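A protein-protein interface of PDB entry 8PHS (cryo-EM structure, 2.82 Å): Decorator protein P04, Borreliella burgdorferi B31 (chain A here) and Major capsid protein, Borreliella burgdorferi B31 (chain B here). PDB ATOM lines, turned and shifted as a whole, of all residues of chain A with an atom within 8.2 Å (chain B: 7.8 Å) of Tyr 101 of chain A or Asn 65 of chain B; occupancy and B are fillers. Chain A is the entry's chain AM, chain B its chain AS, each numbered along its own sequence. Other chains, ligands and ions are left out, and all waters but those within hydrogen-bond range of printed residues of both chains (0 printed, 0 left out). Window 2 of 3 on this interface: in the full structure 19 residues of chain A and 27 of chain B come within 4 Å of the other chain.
Among the printed residues, pairs that only touch across the chains: Cys 98 of chain A with Thr 66 of chain B (3.7 Å), Cys 98 of chain A with Ile 67 of chain B (3.5 Å), Cys 98 of chain A with Ser 68 of chain B (3.996 Å), Ser 99 of chain A with Asn 65 of chain B (3.9 Å), Ser 99 of chain A with Thr 66 of chain B (3.2 Å) and Ser 100 of chain A with Thr 66 of chain B (3.6 Å).
Of chain B, only Asn 65 comes within 4 Å of Tyr 101 of chain A.
Asn 65 of chain B touches just these residues of chain A: Ser 99, Ser 100 and Tyr 101.
Ser 100 of chain A touches just these residues of chain B: Asn 65 (3.4 Å) and Thr 66 (3.6 Å).
Printed residues of chain B within 4 Å of Ser 99 of chain A: Asn 65, Thr 66 and Ile 67.
Of the printed residues of chain B, Cys 98 of chain A touches Thr 66 (3.7 Å), Ile 67 (3.5 Å) and Ser 68 (3.996 Å).
Of the printed residues of chain A, Ile 67 of chain B touches Cys 98 (3.5 Å) and Ser 99 (2.9 Å).
Of the printed residues of chain A, Thr 66 of chain B touches Cys 98 (3.7 Å), Ser 99 (3.2 Å) and Ser 100 (3.6 Å).
Of the printed residues of chain A, Ser 68 of chain B touches Cys 98 (3.996 Å).
Asp 103 of chain A touches none of the printed residues of chain B.
The nearest residue of chain B that does not touch Tyr 101 of chain A is Val 64 of chain B (4.9 Å).
The nearest residue of chain A that does not touch Asn 65 of chain B is Thr 102 of chain A (5.0 Å).
The nearest printed residue of chain A that does not touch Ser 68 of chain B is Ser 99 of chain A (5.0 Å).
The backbone NH of Ile 67 of chain B sits at hydrogen-bond distance from the backbone carbonyl oxygen of Ser 99 of chain A (2.9 Å).
The side-chain amide oxygen of Asn 65 of chain B sits at hydrogen-bond distance from the side-chain hydroxyl of Tyr 101 of chain A, at 2.6 Å.
O of Asn 65 of chain B is in hydrogen-bond range of OG of Ser 100 of chain A (3.4 Å).
Of the 9 printed residues of chain B, 4 touch a printed residue of chain A.
Along chain A the printed residues that touch a printed residue of chain B span positions 98 to 101.
Among the printed residues, 9 pairs touch across the chains.
Among the printed residues, no Asp or Glu carboxylate lies within 4 Å of a Lys or Arg side-chain nitrogen of the other chain.
N of Ser 100 of chain A sits at hydrogen-bond distance from OD2 of Asp 103 of chain A.
N of Ser 68 of chain B lies within hydrogen-bond range of OG1 of Thr 58 of chain B.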
ATOM      1  N   CYS A  98      19.456   4.062   3.328  1.00  0.00           N
ATOM      2  CA  CYS A  98      18.044   4.373   3.141  1.00  0.00           C
ATOM      3  C   CYS A  98      17.959   5.684   2.373  1.00  0.00           C
ATOM      4  O   CYS A  98      18.301   6.742   2.909  1.00  0.00           O
ATOM      5  CB  CYS A  98      17.318   4.478   4.483  1.00  0.00           C
ATOM      6  SG  CYS A  98      17.560   3.063   5.578  1.00  0.00           S
ATOM      7  N   SER A  99      17.508   5.618   1.127  1.00  0.00           N
ATOM      8  CA  SER A  99      17.375   6.813   0.312  1.00  0.00           C
ATOM      9  C   SER A  99      15.975   7.397   0.451  1.00  0.00           C
ATOM     10  O   SER A  99      15.091   6.824   1.090  1.00  0.00           O
ATOM     11  CB  SER A  99      17.677   6.509  -1.156  1.00  0.00           C
ATOM     12  OG  SER A  99      17.585   7.680  -1.945  1.00  0.00           O
ATOM     13  N   SER A 100      15.782   8.560  -0.165  1.00  0.00           N
ATOM     14  CA  SER A 100      14.501   9.248  -0.115  1.00  0.00           C
ATOM     15  C   SER A 100      14.458  10.279  -1.228  1.00  0.00           C
ATOM     16  O   SER A 100      15.410  11.045  -1.399  1.00  0.00           O
ATOM     17  CB  SER A 100      14.292   9.931   1.241  1.00  0.00           C
ATOM     18  OG  SER A 100      13.228  10.864   1.177  1.00  0.00           O
ATOM     19  N   TYR A 101      13.371  10.287  -1.992  1.00  0.00           N
ATOM     20  CA  TYR A 101      13.124  11.431  -2.850  1.00  0.00           C
ATOM     21  C   TYR A 101      12.978  12.674  -1.976  1.00  0.00           C
ATOM     22  O   TYR A 101      12.731  12.587  -0.769  1.00  0.00           O
ATOM     23  CB  TYR A 101      11.888  11.200  -3.723  1.00  0.00           C
ATOM     24  CG  TYR A 101      10.570  11.231  -2.989  1.00  0.00           C
ATOM     25  CD1 TYR A 101      10.101  10.117  -2.311  1.00  0.00           C
ATOM     26  CD2 TYR A 101       9.772  12.365  -3.017  1.00  0.00           C
ATOM     27  CE1 TYR A 101       8.889  10.147  -1.648  1.00  0.00           C
ATOM     28  CE2 TYR A 101       8.562  12.405  -2.359  1.00  0.00           C
ATOM     29  CZ  TYR A 101       8.123  11.295  -1.679  1.00  0.00           C
ATOM     30  OH  TYR A 101       6.913  11.337  -1.027  1.00  0.00           O
ATOM     31  N   THR A 102      13.160  13.841  -2.595  1.00  0.00           N
ATOM     32  CA  THR A 102      13.332  15.137  -1.936  1.00  0.00           C
ATOM     33  C   THR A 102      14.671  15.253  -1.221  1.00  0.00           C
ATOM     34  O   THR A 102      14.825  16.116  -0.348  1.00  0.00           O
ATOM     35  CB  THR A 102      12.207  15.475  -0.948  1.00  0.00           C
ATOM     36  OG1 THR A 102      12.376  14.717   0.257  1.00  0.00           O
ATOM     37  CG2 THR A 102      10.845  15.187  -1.551  1.00  0.00           C
ATOM     38  N   ASP A 103      15.640  14.403  -1.552  1.00  0.00           N
ATOM     39  CA  ASP A 103      17.016  14.596  -1.117  1.00  0.00           C
ATOM     40  C   ASP A 103      17.758  15.395  -2.178  1.00  0.00           C
ATOM     41  O   ASP A 103      17.749  15.029  -3.358  1.00  0.00           O
ATOM     42  CB  ASP A 103      17.717  13.257  -0.876  1.00  0.00           C
ATOM     43  CG  ASP A 103      17.316  12.616   0.437  1.00  0.00           C
ATOM     44  OD1 ASP A 103      16.973  13.355   1.382  1.00  0.00           O
ATOM     45  OD2 ASP A 103      17.363  11.371   0.532  1.00  0.00           O
ATOM     46  N   LYS A 104      18.396  16.483  -1.759  1.00  0.00           N
ATOM     47  CA  LYS A 104      19.075  17.388  -2.676  1.00  0.00           C
ATOM     48  C   LYS A 104      20.491  16.895  -2.941  1.00  0.00           C
ATOM     49  O   LYS A 104      21.256  16.651  -2.004  1.00  0.00           O
ATOM     50  CB  LYS A 104      19.100  18.804  -2.104  1.00  0.00           C
ATOM     51  CG  LYS A 104      19.731  19.840  -3.013  1.00  0.00           C
ATOM     52  CD  LYS A 104      19.332  21.243  -2.589  1.00  0.00           C
ATOM     53  CE  LYS A 104      20.007  22.299  -3.448  1.00  0.00           C
ATOM     54  NZ  LYS A 104      19.536  23.670  -3.110  1.00  0.00           N
ATOM     55  N   THR B  58      11.533  -1.473   4.587  1.00  0.00           N
ATOM     56  CA  THR B  58      10.805  -0.358   5.177  1.00  0.00           C
ATOM     57  C   THR B  58       9.334  -0.720   5.334  1.00  0.00           C
ATOM     58  O   THR B  58       8.693  -1.163   4.375  1.00  0.00           O
ATOM     59  CB  THR B  58      10.949   0.897   4.313  1.00  0.00           C
ATOM     60  OG1 THR B  58      12.312   1.338   4.331  1.00  0.00           O
ATOM     61  CG2 THR B  58      10.054   2.008   4.825  1.00  0.00           C
ATOM     62  N   ILE B  60       5.573   0.010   5.369  1.00  0.00           N
ATOM     63  CA  ILE B  60       4.725   0.992   4.706  1.00  0.00           C
ATOM     64  C   ILE B  60       3.511   1.225   5.599  1.00  0.00           C
ATOM     65  O   ILE B  60       2.551   0.453   5.585  1.00  0.00           O
ATOM     66  CB  ILE B  60       4.321   0.541   3.303  1.00  0.00           C
ATOM     67  CG1 ILE B  60       5.562   0.378   2.431  1.00  0.00           C
ATOM     68  CG2 ILE B  60       3.369   1.545   2.673  1.00  0.00           C
ATOM     69  CD1 ILE B  60       6.373   1.646   2.295  1.00  0.00           C
ATOM     70  N   ASN B  62       1.165   4.725   7.012  1.00  0.00           N
ATOM     71  CA  ASN B  62       0.901   6.175   6.989  1.00  0.00           C
ATOM     72  C   ASN B  62       1.782   6.786   5.894  1.00  0.00           C
ATOM     73  O   ASN B  62       1.893   6.211   4.800  1.00  0.00           O
ATOM     74  CB  ASN B  62       1.096   6.753   8.375  1.00  0.00           C
ATOM     75  CG  ASN B  62       0.022   6.309   9.347  1.00  0.00           C
ATOM     76  OD1 ASN B  62      -0.982   5.717   8.950  1.00  0.00           O
ATOM     77  ND2 ASN B  62       0.229   6.587  10.628  1.00  0.00           N
ATOM     78  N   GLU B  63       2.412   7.931   6.141  1.00  0.00           N
ATOM     79  CA  GLU B  63       3.236   8.605   5.149  1.00  0.00           C
ATOM     80  C   GLU B  63       4.712   8.400   5.459  1.00  0.00           C
ATOM     81  O   GLU B  63       5.134   8.494   6.615  1.00  0.00           O
ATOM     82  CB  GLU B  63       2.921  10.101   5.104  1.00  0.00           C
ATOM     83  CG  GLU B  63       1.461  10.423   4.842  1.00  0.00           C
ATOM     84  CD  GLU B  63       1.168  11.906   4.943  1.00  0.00           C
ATOM     85  OE1 GLU B  63       1.811  12.689   4.214  1.00  0.00           O
ATOM     86  OE2 GLU B  63       0.297  12.289   5.751  1.00  0.00           O
ATOM     87  N   VAL B  64       5.493   8.118   4.419  1.00  0.00           N
ATOM     88  CA  VAL B  64       6.932   7.926   4.565  1.00  0.00           C
ATOM     89  C   VAL B  64       7.579   8.117   3.199  1.00  0.00           C
ATOM     90  O   VAL B  64       7.042   7.688   2.175  1.00  0.00           O
ATOM     91  CB  VAL B  64       7.253   6.539   5.176  1.00  0.00           C
ATOM     92  CG1 VAL B  64       6.737   5.420   4.288  1.00  0.00           C
ATOM     93  CG2 VAL B  64       8.744   6.391   5.422  1.00  0.00           C
ATOM     94  N   ASN B  65       8.732   8.792   3.189  1.00  0.00           N
ATOM     95  CA  ASN B  65       9.499   8.997   1.968  1.00  0.00           C
ATOM     96  C   ASN B  65      10.836   8.273   1.956  1.00  0.00           C
ATOM     97  O   ASN B  65      11.382   8.045   0.873  1.00  0.00           O
ATOM     98  CB  ASN B  65       9.762  10.493   1.733  1.00  0.00           C
ATOM     99  CG  ASN B  65       8.546  11.347   1.997  1.00  0.00           C
ATOM    100  OD1 ASN B  65       7.468  11.097   1.460  1.00  0.00           O
ATOM    101  ND2 ASN B  65       8.715  12.376   2.817  1.00  0.00           N
ATOM    102  N   THR B  66      11.375   7.916   3.117  1.00  0.00           N
ATOM    103  CA  THR B  66      12.678   7.269   3.200  1.00  0.00           C
ATOM    104  C   THR B  66      12.489   5.757   3.174  1.00  0.00           C
ATOM    105  O   THR B  66      11.909   5.183   4.101  1.00  0.00           O
ATOM    106  CB  THR B  66      13.414   7.701   4.465  1.00  0.00           C
ATOM    107  OG1 THR B  66      13.308   9.121   4.613  1.00  0.00           O
ATOM    108  CG2 THR B  66      14.880   7.316   4.385  1.00  0.00           C
ATOM    109  N   ILE B  67      12.984   5.118   2.117  1.00  0.00           N
ATOM    110  CA  ILE B  67      12.820   3.688   1.897  1.00  0.00           C
ATOM    111  C   ILE B  67      14.198   3.055   1.780  1.00  0.00           C
ATOM    112  O   ILE B  67      15.138   3.682   1.280  1.00  0.00           O
ATOM    113  CB  ILE B  67      11.981   3.400   0.634  1.00  0.00           C
ATOM    114  CG1 ILE B  67      10.768   4.332   0.568  1.00  0.00           C
ATOM    115  CG2 ILE B  67      11.530   1.952   0.608  1.00  0.00           C
ATOM    116  CD1 ILE B  67       9.740   4.073   1.640  1.00  0.00           C
ATOM    117  N   SER B  68      14.318   1.817   2.254  1.00  0.00           N
ATOM    118  CA  SER B  68      15.570   1.085   2.118  1.00  0.00           C
ATOM    119  C   SER B  68      15.870   0.822   0.649  1.00  0.00           C
ATOM    120  O   SER B  68      14.966   0.721  -0.185  1.00  0.00           O
ATOM    121  CB  SER B  68      15.506  -0.232   2.886  1.00  0.00           C
ATOM    122  OG  SER B  68      15.356  -0.005   4.276  1.00  0.00           O
